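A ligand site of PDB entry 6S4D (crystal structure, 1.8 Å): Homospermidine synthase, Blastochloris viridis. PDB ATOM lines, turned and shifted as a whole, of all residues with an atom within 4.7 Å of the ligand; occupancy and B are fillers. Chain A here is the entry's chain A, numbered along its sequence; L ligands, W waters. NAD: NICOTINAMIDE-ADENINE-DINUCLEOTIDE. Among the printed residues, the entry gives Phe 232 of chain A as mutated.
A nitrogen (N6A) of the ligand is in hydrogen-bond range of the backbone carbonyl oxygen (O) of Val 69, at 3.0 Å.
The backbone carbonyl oxygen (O) of Asn 165 lies within hydrogen-bond range of a nitrogen (N7N) of the ligand (3.4 Å).
An oxygen (O7N) of the ligand sits at hydrogen-bond distance from the backbone NH of Ala 164.
The backbone NH (N) of Ile 25 is in hydrogen-bond range of an oxygen (O1N) of the ligand, at 2.9 Å.
The side-chain carboxylate (OD2) of Asp 48 lies within hydrogen-bond range of an oxygen (O3B) of the ligand, 2.4 Å away.
The backbone carbonyl oxygen (O) of Thr 117 lies within hydrogen-bond range of a nitrogen (N7N) of the ligand (3.0 Å).
A nitrogen (N1A) of the ligand lies within hydrogen-bond range of the backbone NH (N) of Val 69 (3.1 Å).
OG1 of Thr 117 is in hydrogen-bond range of O4D of the ligand (2.9 Å).
The backbone NH of Asn 165 is in hydrogen-bond range of an oxygen (O7N) of the ligand (2.9 Å).
The side-chain hydroxyl (OG) of Ser 24 sits at hydrogen-bond distance from an oxygen (O2N) of the ligand.
The backbone NH (N) of Ser 24 sits at hydrogen-bond distance from an oxygen (O1N) of the ligand (3.0 Å).
A nitrogen (N7N) of the ligand lies within hydrogen-bond range of the backbone carbonyl oxygen (O) of Pro 166 (3.2 Å).
The backbone carbonyl oxygen (O) of Ser 95 lies within hydrogen-bond range of an oxygen (O3D) of the ligand.
An oxygen (O2N) of the ligand is in hydrogen-bond range of the backbone NH (N) of Ser 233 (3.1 Å).
An oxygen (O2A) of the ligand lies within hydrogen-bond range of the side-chain hydroxyl (OG) of Ser 233 (3.0 Å).
OD1 of Asp 48 sits at hydrogen-bond distance from N of Ser 50 (2.8 Å).
OG of Ser 233 lies within hydrogen-bond range of N of Gly 236, at 2.8 Å.
N of Leu 94 sits at hydrogen-bond distance from O of Ile 20.
N of Phe 22 lies within hydrogen-bond range of OD2 of Asp 48.
The backbone carbonyl oxygen of Gly 23 lies close to the guanidinium group of Arg 27 (3.1 Å).
O of Ile 20 lies within hydrogen-bond range of N of Ser 95 (3.4 Å).
The backbone NH of Gln 67 lies within hydrogen-bond range of the backbone carbonyl oxygen of Asp 48 (3.4 Å).
The side-chain hydroxyl (OG) of Ser 95 sits at hydrogen-bond distance from the side-chain hydroxyl (OG1) of Thr 98, at 2.6 Å.
A nitrogen (N7A) of the ligand lies close to the backbone carbonyl oxygen of Val 96 (3.3 Å).
Residues that only touch the ligand: Gly 23 (3.2 Å), Leu 94 (3.4 Å), Pro 49 (3.4 Å), Ile 353 (3.4 Å), Val 403 (3.5 Å), Ala 68 (3.5 Å), Val 118 (3.5 Å), Thr 98 (3.6 Å), Phe 22 (3.7 Å), Gly 163 (3.7 Å), Phe 232 (3.8 Å), Ser 50 (3.9 Å) and Ile 20 (3.9 Å).
Hydrophobic or aromatic side chains within 4 Å of the ligand: Ile 20, Ile 25, Pro 49, Ala 68, Val 69, Val 96, Val 118, Ala 164, Pro 166, Phe 232, Ile 353 and Val 403.
24 residues have an atom within 4 Å of the ligand: Ile 20, Phe 22, Gly 23, Ser 24, Ile 25, Asp 48, Pro 49, Ser 50, Ala 68, Val 69, Leu 94, Ser 95, Val 96, Thr 98, Thr 117, Val 118, Gly 163, Ala 164, Asn 165, Pro 166, Phe 232, Ser 233, Ile 353 and Val 403.
Water W11 lies within hydrogen-bond range of O1N of the ligand (2.8 Å), N of Gly 23 (2.8 Å), N of Gly 26 (2.9 Å) and O of Leu 94 (2.9 Å).
Water W12 lies within hydrogen-bond range of OD2 of Asp 97 (2.6 Å) and N7A of the ligand (2.8 Å).
Water W7 lies within hydrogen-bond range of OG of Ser 50, O3B of the ligand and NH2 of Arg 27.
Water W10 bridges OE1 of Glu 120 (2.7 Å) and O2D of the ligand (2.9 Å).
Water W5 lies within hydrogen-bond range of the backbone carbonyl oxygen (O) of Asp 97 (2.7 Å), the backbone carbonyl oxygen (O) of Val 69 (2.7 Å) and a nitrogen (N6A) of the ligand (3.4 Å).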
ATOM      1  N   ILE A  20      16.317   5.299  18.669  1.00  0.00           N
ATOM      2  CA  ILE A  20      15.456   4.137  18.827  1.00  0.00           C
ATOM      3  C   ILE A  20      14.460   4.498  19.920  1.00  0.00           C
ATOM      4  O   ILE A  20      14.827   4.704  21.075  1.00  0.00           O
ATOM      5  CB  ILE A  20      16.268   2.889  19.176  1.00  0.00           C
ATOM      6  CG1 ILE A  20      17.420   2.730  18.185  1.00  0.00           C
ATOM      7  CG2 ILE A  20      15.370   1.656  19.192  1.00  0.00           C
ATOM      8  CD1 ILE A  20      18.254   1.510  18.425  1.00  0.00           C
ATOM      9  N   GLY A  21      13.188   4.598  19.548  1.00  0.00           N
ATOM     10  CA  GLY A  21      12.152   4.925  20.512  1.00  0.00           C
ATOM     11  C   GLY A  21      11.862   6.411  20.503  1.00  0.00           C
ATOM     12  O   GLY A  21      12.785   7.223  20.574  1.00  0.00           O
ATOM     13  N   PHE A  22      10.590   6.777  20.404  1.00  0.00           N
ATOM     14  CA  PHE A  22      10.200   8.172  20.356  1.00  0.00           C
ATOM     15  C   PHE A  22       8.985   8.350  21.274  1.00  0.00           C
ATOM     16  O   PHE A  22       7.890   8.705  20.856  1.00  0.00           O
ATOM     17  CB  PHE A  22       9.917   8.586  18.903  1.00  0.00           C
ATOM     18  CG  PHE A  22       9.968  10.062  18.674  1.00  0.00           C
ATOM     19  CD1 PHE A  22      11.148  10.773  18.887  1.00  0.00           C
ATOM     20  CD2 PHE A  22       8.850  10.746  18.219  1.00  0.00           C
ATOM     21  CE1 PHE A  22      11.199  12.133  18.684  1.00  0.00           C
ATOM     22  CE2 PHE A  22       8.896  12.120  18.007  1.00  0.00           C
ATOM     23  CZ  PHE A  22      10.086  12.814  18.242  1.00  0.00           C
ATOM     24  N   GLY A  23       9.194   8.062  22.558  1.00  0.00           N
ATOM     25  CA  GLY A  23       8.184   8.226  23.602  1.00  0.00           C
ATOM     26  C   GLY A  23       8.379   9.566  24.290  1.00  0.00           C
ATOM     27  O   GLY A  23       8.749  10.534  23.645  1.00  0.00           O
ATOM     28  N   SER A  24       8.136   9.635  25.623  1.00  0.00           N
ATOM     29  CA  SER A  24       8.235  10.940  26.295  1.00  0.00           C
ATOM     30  C   SER A  24       9.673  11.448  26.335  1.00  0.00           C
ATOM     31  O   SER A  24       9.915  12.659  26.244  1.00  0.00           O
ATOM     32  CB  SER A  24       7.626  10.852  27.710  1.00  0.00           C
ATOM     33  OG  SER A  24       8.559  10.392  28.695  1.00  0.00           O
ATOM     34  N   ILE A  25      10.657  10.558  26.460  1.00  0.00           N
ATOM     35  CA  ILE A  25      12.040  11.016  26.536  1.00  0.00           C
ATOM     36  C   ILE A  25      12.576  11.323  25.145  1.00  0.00           C
ATOM     37  O   ILE A  25      13.244  12.343  24.950  1.00  0.00           O
ATOM     38  CB  ILE A  25      12.931   9.984  27.261  1.00  0.00           C
ATOM     39  CG1 ILE A  25      12.407   9.682  28.673  1.00  0.00           C
ATOM     40  CG2 ILE A  25      14.372  10.499  27.342  1.00  0.00           C
ATOM     41  CD1 ILE A  25      12.157  10.931  29.571  1.00  0.00           C
ATOM     42  N   GLY A  26      12.311  10.447  24.173  1.00  0.00           N
ATOM     43  CA  GLY A  26      12.713  10.745  22.804  1.00  0.00           C
ATOM     44  C   GLY A  26      12.179  12.088  22.314  1.00  0.00           C
ATOM     45  O   GLY A  26      12.897  12.852  21.675  1.00  0.00           O
ATOM     46  N   ARG A  27      10.927  12.394  22.643  1.00  0.00           N
ATOM     47  CA  ARG A  27      10.318  13.641  22.197  1.00  0.00           C
ATOM     48  C   ARG A  27      10.937  14.856  22.865  1.00  0.00           C
ATOM     49  O   ARG A  27      10.927  15.948  22.286  1.00  0.00           O
ATOM     50  CB  ARG A  27       8.809  13.609  22.450  1.00  0.00           C
ATOM     51  CG  ARG A  27       8.068  12.600  21.585  1.00  0.00           C
ATOM     52  CD  ARG A  27       6.740  12.152  22.198  1.00  0.00           C
ATOM     53  NE  ARG A  27       6.341  10.858  21.661  1.00  0.00           N
ATOM     54  CZ  ARG A  27       5.165  10.276  21.872  1.00  0.00           C
ATOM     55  NH1 ARG A  27       4.244  10.889  22.625  1.00  0.00           N
ATOM     56  NH2 ARG A  27       4.910   9.091  21.333  1.00  0.00           N
ATOM     57  N   ILE A  47      13.157   5.349  14.982  1.00  0.00           N
ATOM     58  CA  ILE A  47      12.580   4.016  14.850  1.00  0.00           C
ATOM     59  C   ILE A  47      11.623   3.791  16.018  1.00  0.00           C
ATOM     60  O   ILE A  47      12.031   3.829  17.177  1.00  0.00           O
ATOM     61  CB  ILE A  47      13.667   2.926  14.843  1.00  0.00           C
ATOM     62  CG1 ILE A  47      14.788   3.294  13.887  1.00  0.00           C
ATOM     63  CG2 ILE A  47      13.063   1.579  14.466  1.00  0.00           C
ATOM     64  CD1 ILE A  47      15.940   2.383  13.961  1.00  0.00           C
ATOM     65  N   ASP A  48      10.358   3.520  15.708  1.00  0.00           N
ATOM     66  CA  ASP A  48       9.385   3.288  16.771  1.00  0.00           C
ATOM     67  C   ASP A  48       8.199   2.575  16.160  1.00  0.00           C
ATOM     68  O   ASP A  48       7.798   2.915  15.047  1.00  0.00           O
ATOM     69  CB  ASP A  48       8.968   4.604  17.429  1.00  0.00           C
ATOM     70  CG  ASP A  48       8.116   4.401  18.685  1.00  0.00           C
ATOM     71  OD1 ASP A  48       7.085   3.708  18.581  1.00  0.00           O
ATOM     72  OD2 ASP A  48       8.485   4.918  19.772  1.00  0.00           O
ATOM     73  N   PRO A  49       7.625   1.570  16.828  1.00  0.00           N
ATOM     74  CA  PRO A  49       6.503   0.832  16.217  1.00  0.00           C
ATOM     75  C   PRO A  49       5.155   1.538  16.283  1.00  0.00           C
ATOM     76  O   PRO A  49       4.217   1.080  15.616  1.00  0.00           O
ATOM     77  CB  PRO A  49       6.473  -0.471  17.026  1.00  0.00           C
ATOM     78  CG  PRO A  49       6.984  -0.087  18.349  1.00  0.00           C
ATOM     79  CD  PRO A  49       8.061   0.927  18.091  1.00  0.00           C
ATOM     80  N   SER A  50       5.002   2.627  17.025  1.00  0.00           N
ATOM     81  CA  SER A  50       3.681   3.190  17.264  1.00  0.00           C
ATOM     82  C   SER A  50       3.304   4.251  16.221  1.00  0.00           C
ATOM     83  O   SER A  50       4.144   4.989  15.718  1.00  0.00           O
ATOM     84  CB  SER A  50       3.587   3.815  18.655  1.00  0.00           C
ATOM     85  OG  SER A  50       3.935   5.185  18.623  1.00  0.00           O
ATOM     86  N   GLN A  67       8.911   0.373  13.015  1.00  0.00           N
ATOM     87  CA  GLN A  67       9.295  -1.001  13.307  1.00  0.00           C
ATOM     88  C   GLN A  67       9.628  -1.099  14.779  1.00  0.00           C
ATOM     89  O   GLN A  67      10.187  -0.168  15.363  1.00  0.00           O
ATOM     90  CB  GLN A  67      10.505  -1.452  12.469  1.00  0.00           C
ATOM     91  CG  GLN A  67      10.223  -1.642  10.983  1.00  0.00           C
ATOM     92  CD  GLN A  67       9.473  -2.923  10.686  1.00  0.00           C
ATOM     93  OE1 GLN A  67       9.432  -3.839  11.511  1.00  0.00           O
ATOM     94  NE2 GLN A  67       8.881  -3.006   9.487  1.00  0.00           N
ATOM     95  N   ALA A  68       9.245  -2.213  15.382  1.00  0.00           N
ATOM     96  CA  ALA A  68       9.772  -2.606  16.683  1.00  0.00           C
ATOM     97  C   ALA A  68      11.099  -3.301  16.456  1.00  0.00           C
ATOM     98  O   ALA A  68      11.216  -4.199  15.614  1.00  0.00           O
ATOM     99  CB  ALA A  68       8.787  -3.539  17.405  1.00  0.00           C
ATOM    100  N   VAL A  69      12.123  -2.853  17.176  1.00  0.00           N
ATOM    101  CA  VAL A  69      13.414  -3.530  17.163  1.00  0.00           C
ATOM    102  C   VAL A  69      13.305  -4.772  18.050  1.00  0.00           C
ATOM    103  O   VAL A  69      12.882  -4.669  19.208  1.00  0.00           O
ATOM    104  CB  VAL A  69      14.530  -2.593  17.658  1.00  0.00           C
ATOM    105  CG1 VAL A  69      15.894  -3.294  17.673  1.00  0.00           C
ATOM    106  CG2 VAL A  69      14.584  -1.350  16.814  1.00  0.00           C
ATOM    107  N   LEU A  94      16.369   5.169  23.408  1.00  0.00           N
ATOM    108  CA  LEU A  94      15.411   5.644  24.397  1.00  0.00           C
ATOM    109  C   LEU A  94      14.140   4.810  24.328  1.00  0.00           C
ATOM    110  O   LEU A  94      13.027   5.331  24.408  1.00  0.00           O
ATOM    111  CB  LEU A  94      15.124   7.138  24.179  1.00  0.00           C
ATOM    112  CG  LEU A  94      16.360   8.033  24.123  1.00  0.00           C
ATOM    113  CD1 LEU A  94      16.001   9.457  23.721  1.00  0.00           C
ATOM    114  CD2 LEU A  94      17.087   8.035  25.468  1.00  0.00           C
ATOM    115  N   SER A  95      14.286   3.510  24.227  1.00  0.00           N
ATOM    116  CA  SER A  95      13.167   2.616  23.974  1.00  0.00           C
ATOM    117  C   SER A  95      12.834   1.778  25.203  1.00  0.00           C
ATOM    118  O   SER A  95      13.558   1.779  26.212  1.00  0.00           O
ATOM    119  CB  SER A  95      13.510   1.694  22.800  1.00  0.00           C
ATOM    120  OG  SER A  95      14.631   0.898  23.117  1.00  0.00           O
ATOM    121  N   VAL A  96      11.704   1.089  25.120  1.00  0.00           N
ATOM    122  CA  VAL A  96      11.393  -0.035  25.985  1.00  0.00           C
ATOM    123  C   VAL A  96      11.427  -1.299  25.136  1.00  0.00           C
ATOM    124  O   VAL A  96      11.343  -1.270  23.898  1.00  0.00           O
ATOM    125  CB  VAL A  96      10.031   0.107  26.694  1.00  0.00           C
ATOM    126  CG1 VAL A  96      10.055   1.307  27.619  1.00  0.00           C
ATOM    127  CG2 VAL A  96       8.893   0.237  25.688  1.00  0.00           C
ATOM    128  N   ASP A  97      11.565  -2.434  25.811  1.00  0.00           N
ATOM    129  CA  ASP A  97      11.421  -3.763  25.226  1.00  0.00           C
ATOM    130  C   ASP A  97      12.584  -4.177  24.331  1.00  0.00           C
ATOM    131  O   ASP A  97      12.469  -5.185  23.624  1.00  0.00           O
ATOM    132  CB  ASP A  97      10.124  -3.874  24.413  1.00  0.00           C
ATOM    133  CG  ASP A  97       8.884  -3.764  25.280  1.00  0.00           C
ATOM    134  OD1 ASP A  97       9.027  -3.787  26.515  1.00  0.00           O
ATOM    135  OD2 ASP A  97       7.764  -3.668  24.712  1.00  0.00           O
ATOM    136  N   THR A  98      13.703  -3.447  24.352  1.00  0.00           N
ATOM    137  CA  THR A  98      14.881  -3.795  23.574  1.00  0.00           C
ATOM    138  C   THR A  98      16.072  -4.060  24.495  1.00  0.00           C
ATOM    139  O   THR A  98      16.163  -3.545  25.604  1.00  0.00           O
ATOM    140  CB  THR A  98      15.243  -2.665  22.583  1.00  0.00           C
ATOM    141  OG1 THR A  98      15.658  -1.494  23.295  1.00  0.00           O
ATOM    142  CG2 THR A  98      14.033  -2.302  21.715  1.00  0.00           C
ATOM    143  N   THR A 117      19.450   5.044  28.732  1.00  0.00           N
ATOM    144  CA  THR A 117      19.096   5.519  30.059  1.00  0.00           C
ATOM    145  C   THR A 117      18.695   4.384  30.992  1.00  0.00           C
ATOM    146  O   THR A 117      18.166   4.642  32.072  1.00  0.00           O
ATOM    147  CB  THR A 117      17.949   6.533  29.993  1.00  0.00           C
ATOM    148  OG1 THR A 117      16.746   5.859  29.604  1.00  0.00           O
ATOM    149  CG2 THR A 117      18.249   7.644  29.010  1.00  0.00           C
ATOM    150  N   VAL A 118      18.922   3.139  30.597  1.00  0.00           N
ATOM    151  CA  VAL A 118      18.485   1.982  31.371  1.00  0.00           C
ATOM    152  C   VAL A 118      19.072   0.733  30.743  1.00  0.00           C
ATOM    153  O   VAL A 118      19.280   0.684  29.531  1.00  0.00           O
ATOM    154  CB  VAL A 118      16.942   1.900  31.456  1.00  0.00           C
ATOM    155  CG1 VAL A 118      16.305   1.810  30.051  1.00  0.00           C
ATOM    156  CG2 VAL A 118      16.518   0.735  32.317  1.00  0.00           C
ATOM    157  N   GLU A 120      17.884  -2.299  29.686  1.00  0.00           N
ATOM    158  CA  GLU A 120      16.626  -2.907  29.307  1.00  0.00           C
ATOM    159  C   GLU A 120      16.882  -4.279  28.673  1.00  0.00           C
ATOM    160  O   GLU A 120      17.882  -4.454  27.967  1.00  0.00           O
ATOM    161  CB  GLU A 120      15.885  -2.005  28.321  1.00  0.00           C
ATOM    162  CG  GLU A 120      14.486  -2.476  27.910  1.00  0.00           C
ATOM    163  CD  GLU A 120      13.418  -2.095  28.925  1.00  0.00           C
ATOM    164  OE1 GLU A 120      13.803  -1.659  30.037  1.00  0.00           O
ATOM    165  OE2 GLU A 120      12.204  -2.219  28.604  1.00  0.00           O
ATOM    166  N   GLY A 163      20.529   8.855  32.080  1.00  0.00           N
ATOM    167  CA  GLY A 163      19.385   9.742  32.168  1.00  0.00           C
ATOM    168  C   GLY A 163      19.451  10.585  33.429  1.00  0.00           C
ATOM    169  O   GLY A 163      20.542  10.976  33.839  1.00  0.00           O
ATOM    170  N   ALA A 164      18.320  10.883  34.056  1.00  0.00           N
ATOM    171  CA  ALA A 164      18.331  11.625  35.320  1.00  0.00           C
ATOM    172  C   ALA A 164      18.726  10.744  36.492  1.00  0.00           C
ATOM    173  O   ALA A 164      19.555  11.134  37.327  1.00  0.00           O
ATOM    174  CB  ALA A 164      16.956  12.238  35.587  1.00  0.00           C
ATOM    175  N   ASN A 165      18.141   9.566  36.584  1.00  0.00           N
ATOM    176  CA  ASN A 165      18.472   8.609  37.622  1.00  0.00           C
ATOM    177  C   ASN A 165      18.044   7.232  37.132  1.00  0.00           C
ATOM    178  O   ASN A 165      16.837   6.973  37.048  1.00  0.00           O
ATOM    179  CB  ASN A 165      17.835   8.988  38.967  1.00  0.00           C
ATOM    180  CG  ASN A 165      16.323   9.206  38.900  1.00  0.00           C
ATOM    181  OD1 ASN A 165      15.784   9.774  37.948  1.00  0.00           O
ATOM    182  ND2 ASN A 165      15.625   8.753  39.935  1.00  0.00           N
ATOM    183  N   PRO A 166      18.985   6.362  36.730  1.00  0.00           N
ATOM    184  CA  PRO A 166      20.447   6.526  36.755  1.00  0.00           C
ATOM    185  C   PRO A 166      20.921   7.600  35.801  1.00  0.00           C
ATOM    186  O   PRO A 166      20.247   7.915  34.810  1.00  0.00           O
ATOM    187  CB  PRO A 166      20.974   5.144  36.343  1.00  0.00           C
ATOM    188  CG  PRO A 166      19.886   4.589  35.487  1.00  0.00           C
ATOM    189  CD  PRO A 166      18.604   5.084  36.090  1.00  0.00           C
ATOM    190  N   PHE A 232       6.309  10.042  33.200  1.00  0.00           N
ATOM    191  CA  PHE A 232       7.204   9.402  32.244  1.00  0.00           C
ATOM    192  C   PHE A 232       6.685   7.977  32.023  1.00  0.00           C
ATOM    193  O   PHE A 232       5.654   7.583  32.586  1.00  0.00           O
ATOM    194  CB  PHE A 232       8.643   9.429  32.752  1.00  0.00           C
ATOM    195  CG  PHE A 232       8.828   8.630  34.002  1.00  0.00           C
ATOM    196  CD1 PHE A 232       8.459   9.138  35.228  1.00  0.00           C
ATOM    197  CD2 PHE A 232       9.305   7.337  33.933  1.00  0.00           C
ATOM    198  CE1 PHE A 232       8.610   8.393  36.374  1.00  0.00           C
ATOM    199  CE2 PHE A 232       9.465   6.591  35.083  1.00  0.00           C
ATOM    200  CZ  PHE A 232       9.114   7.106  36.297  1.00  0.00           C
ATOM    201  N   SER A 233       7.423   7.202  31.231  1.00  0.00           N
ATOM    202  CA  SER A 233       7.012   5.869  30.803  1.00  0.00           C
ATOM    203  C   SER A 233       6.174   5.154  31.853  1.00  0.00           C
ATOM    204  O   SER A 233       6.645   4.883  32.970  1.00  0.00           O
ATOM    205  CB  SER A 233       8.230   5.000  30.498  1.00  0.00           C
ATOM    206  OG  SER A 233       7.840   3.769  29.907  1.00  0.00           O
ATOM    207  N   GLY A 236       7.575   1.413  31.457  1.00  0.00           N
ATOM    208  CA  GLY A 236       8.870   1.265  32.095  1.00  0.00           C
ATOM    209  C   GLY A 236       8.790   1.373  33.600  1.00  0.00           C
ATOM    210  O   GLY A 236       9.455   0.626  34.333  1.00  0.00           O
ATOM    211  N   ILE A 353       0.644   9.388  30.071  1.00  0.00           N
ATOM    212  CA  ILE A 353       1.734  10.210  30.554  1.00  0.00           C
ATOM    213  C   ILE A 353       1.282  11.660  30.484  1.00  0.00           C
ATOM    214  O   ILE A 353       0.760  12.098  29.453  1.00  0.00           O
ATOM    215  CB  ILE A 353       3.006   9.987  29.719  1.00  0.00           C
ATOM    216  CG1 ILE A 353       3.407   8.513  29.754  1.00  0.00           C
ATOM    217  CG2 ILE A 353       4.115  10.906  30.203  1.00  0.00           C
ATOM    218  CD1 ILE A 353       4.582   8.168  28.845  1.00  0.00           C
ATOM    219  N   VAL A 403      15.813  14.262  32.363  1.00  0.00           N
ATOM    220  CA  VAL A 403      16.341  13.079  31.683  1.00  0.00           C
ATOM    221  C   VAL A 403      16.986  13.469  30.357  1.00  0.00           C
ATOM    222  O   VAL A 403      18.116  13.059  30.055  1.00  0.00           O
ATOM    223  CB  VAL A 403      15.215  12.045  31.466  1.00  0.00           C
ATOM    224  CG1 VAL A 403      15.775  10.796  30.801  1.00  0.00           C
ATOM    225  CG2 VAL A 403      14.510  11.675  32.781  1.00  0.00           C
HETATM  226  PA  NAD L   1       7.673   5.758  26.759  1.00  0.00           P
HETATM  227  O1A NAD L   1       7.074   7.016  26.775  1.00  0.00           O
HETATM  228  O2A NAD L   1       6.959   4.651  27.194  1.00  0.00           O
HETATM  229  O5B NAD L   1       8.084   5.483  25.300  1.00  0.00           O
HETATM  230  C5B NAD L   1       8.595   4.283  24.880  1.00  0.00           C
HETATM  231  C4B NAD L   1       8.693   4.221  23.367  1.00  0.00           C
HETATM  232  O4B NAD L   1       9.341   3.050  22.992  1.00  0.00           O
HETATM  233  C3B NAD L   1       7.307   4.174  22.747  1.00  0.00           C
HETATM  234  O3B NAD L   1       7.191   5.214  21.830  1.00  0.00           O
HETATM  235  C2B NAD L   1       7.247   2.758  22.159  1.00  0.00           C
HETATM  236  O2B NAD L   1       6.496   2.635  21.004  1.00  0.00           O
HETATM  237  C1B NAD L   1       8.689   2.477  21.903  1.00  0.00           C
HETATM  238  N9A NAD L   1       8.931   1.063  21.723  1.00  0.00           N
HETATM  239  C8A NAD L   1       8.296   0.064  22.266  1.00  0.00           C
HETATM  240  N7A NAD L   1       8.817  -1.088  21.833  1.00  0.00           N
HETATM  241  C5A NAD L   1       9.790  -0.800  21.008  1.00  0.00           C
HETATM  242  C6A NAD L   1      10.745  -1.534  20.213  1.00  0.00           C
HETATM  243  N6A NAD L   1      10.742  -2.847  20.232  1.00  0.00           N
HETATM  244  N1A NAD L   1      11.600  -0.825  19.492  1.00  0.00           N
HETATM  245  C2A NAD L   1      11.616   0.484  19.489  1.00  0.00           C
HETATM  246  N3A NAD L   1      10.765   1.187  20.183  1.00  0.00           N
HETATM  247  C4A NAD L   1       9.870   0.622  20.940  1.00  0.00           C
HETATM  248  O3  NAD L   1       8.997   5.807  27.573  1.00  0.00           O
HETATM  249  PN  NAD L   1       9.898   7.035  27.940  1.00  0.00           P
HETATM  250  O1N NAD L   1      10.168   7.700  26.765  1.00  0.00           O
HETATM  251  O2N NAD L   1       9.395   7.797  28.980  1.00  0.00           O
HETATM  252  O5D NAD L   1      11.168   6.338  28.469  1.00  0.00           O
HETATM  253  C5D NAD L   1      12.090   5.743  27.604  1.00  0.00           C
HETATM  254  C4D NAD L   1      13.073   4.892  28.353  1.00  0.00           C
HETATM  255  O4D NAD L   1      13.842   5.664  29.235  1.00  0.00           O
HETATM  256  C3D NAD L   1      12.394   3.832  29.183  1.00  0.00           C
HETATM  257  O3D NAD L   1      13.024   2.607  29.017  1.00  0.00           O
HETATM  258  C2D NAD L   1      12.543   4.330  30.603  1.00  0.00           C
HETATM  259  O2D NAD L   1      12.580   3.275  31.543  1.00  0.00           O
HETATM  260  C1D NAD L   1      13.824   5.137  30.535  1.00  0.00           C
HETATM  261  N1N NAD L   1      13.891   6.228  31.512  1.00  0.00           N
HETATM  262  C2N NAD L   1      14.998   6.493  32.167  1.00  0.00           C
HETATM  263  C3N NAD L   1      15.069   7.501  33.078  1.00  0.00           C
HETATM  264  C7N NAD L   1      16.326   7.830  33.801  1.00  0.00           C
HETATM  265  O7N NAD L   1      16.372   8.835  34.375  1.00  0.00           O
HETATM  266  N7N NAD L   1      17.377   7.040  33.714  1.00  0.00           N
HETATM  267  C4N NAD L   1      13.955   8.265  33.313  1.00  0.00           C
HETATM  268  C5N NAD L   1      12.837   7.984  32.609  1.00  0.00           C
HETATM  269  C6N NAD L   1      12.835   6.956  31.714  1.00  0.00           C
HETATM  270  O   HOH W   1       4.985   7.885  25.231  1.00  0.00           O
HETATM  271  O   HOH W   2       5.640   2.797  25.708  1.00  0.00           O
HETATM  272  O   HOH W   3       4.361   3.994  28.820  1.00  0.00           O
HETATM  273  O   HOH W   4       5.740  -0.594  24.331  1.00  0.00           O
HETATM  274  O   HOH W   5      11.624  -5.980  21.226  1.00  0.00           O
HETATM  275  O   HOH W   6       8.967  -5.466  20.834  1.00  0.00           O
HETATM  276  O   HOH W   7       4.473   5.991  21.308  1.00  0.00           O
HETATM  277  O   HOH W   8       4.173   1.196  21.368  1.00  0.00           O
HETATM  278  O   HOH W   9      11.217   3.843  33.720  1.00  0.00           O
HETATM  279  O   HOH W  10      12.459   0.431  30.983  1.00  0.00           O
HETATM  280  O   HOH W  11      11.349   7.711  24.280  1.00  0.00           O
HETATM  281  O   HOH W  12       7.513  -3.596  22.175  1.00  0.00           O
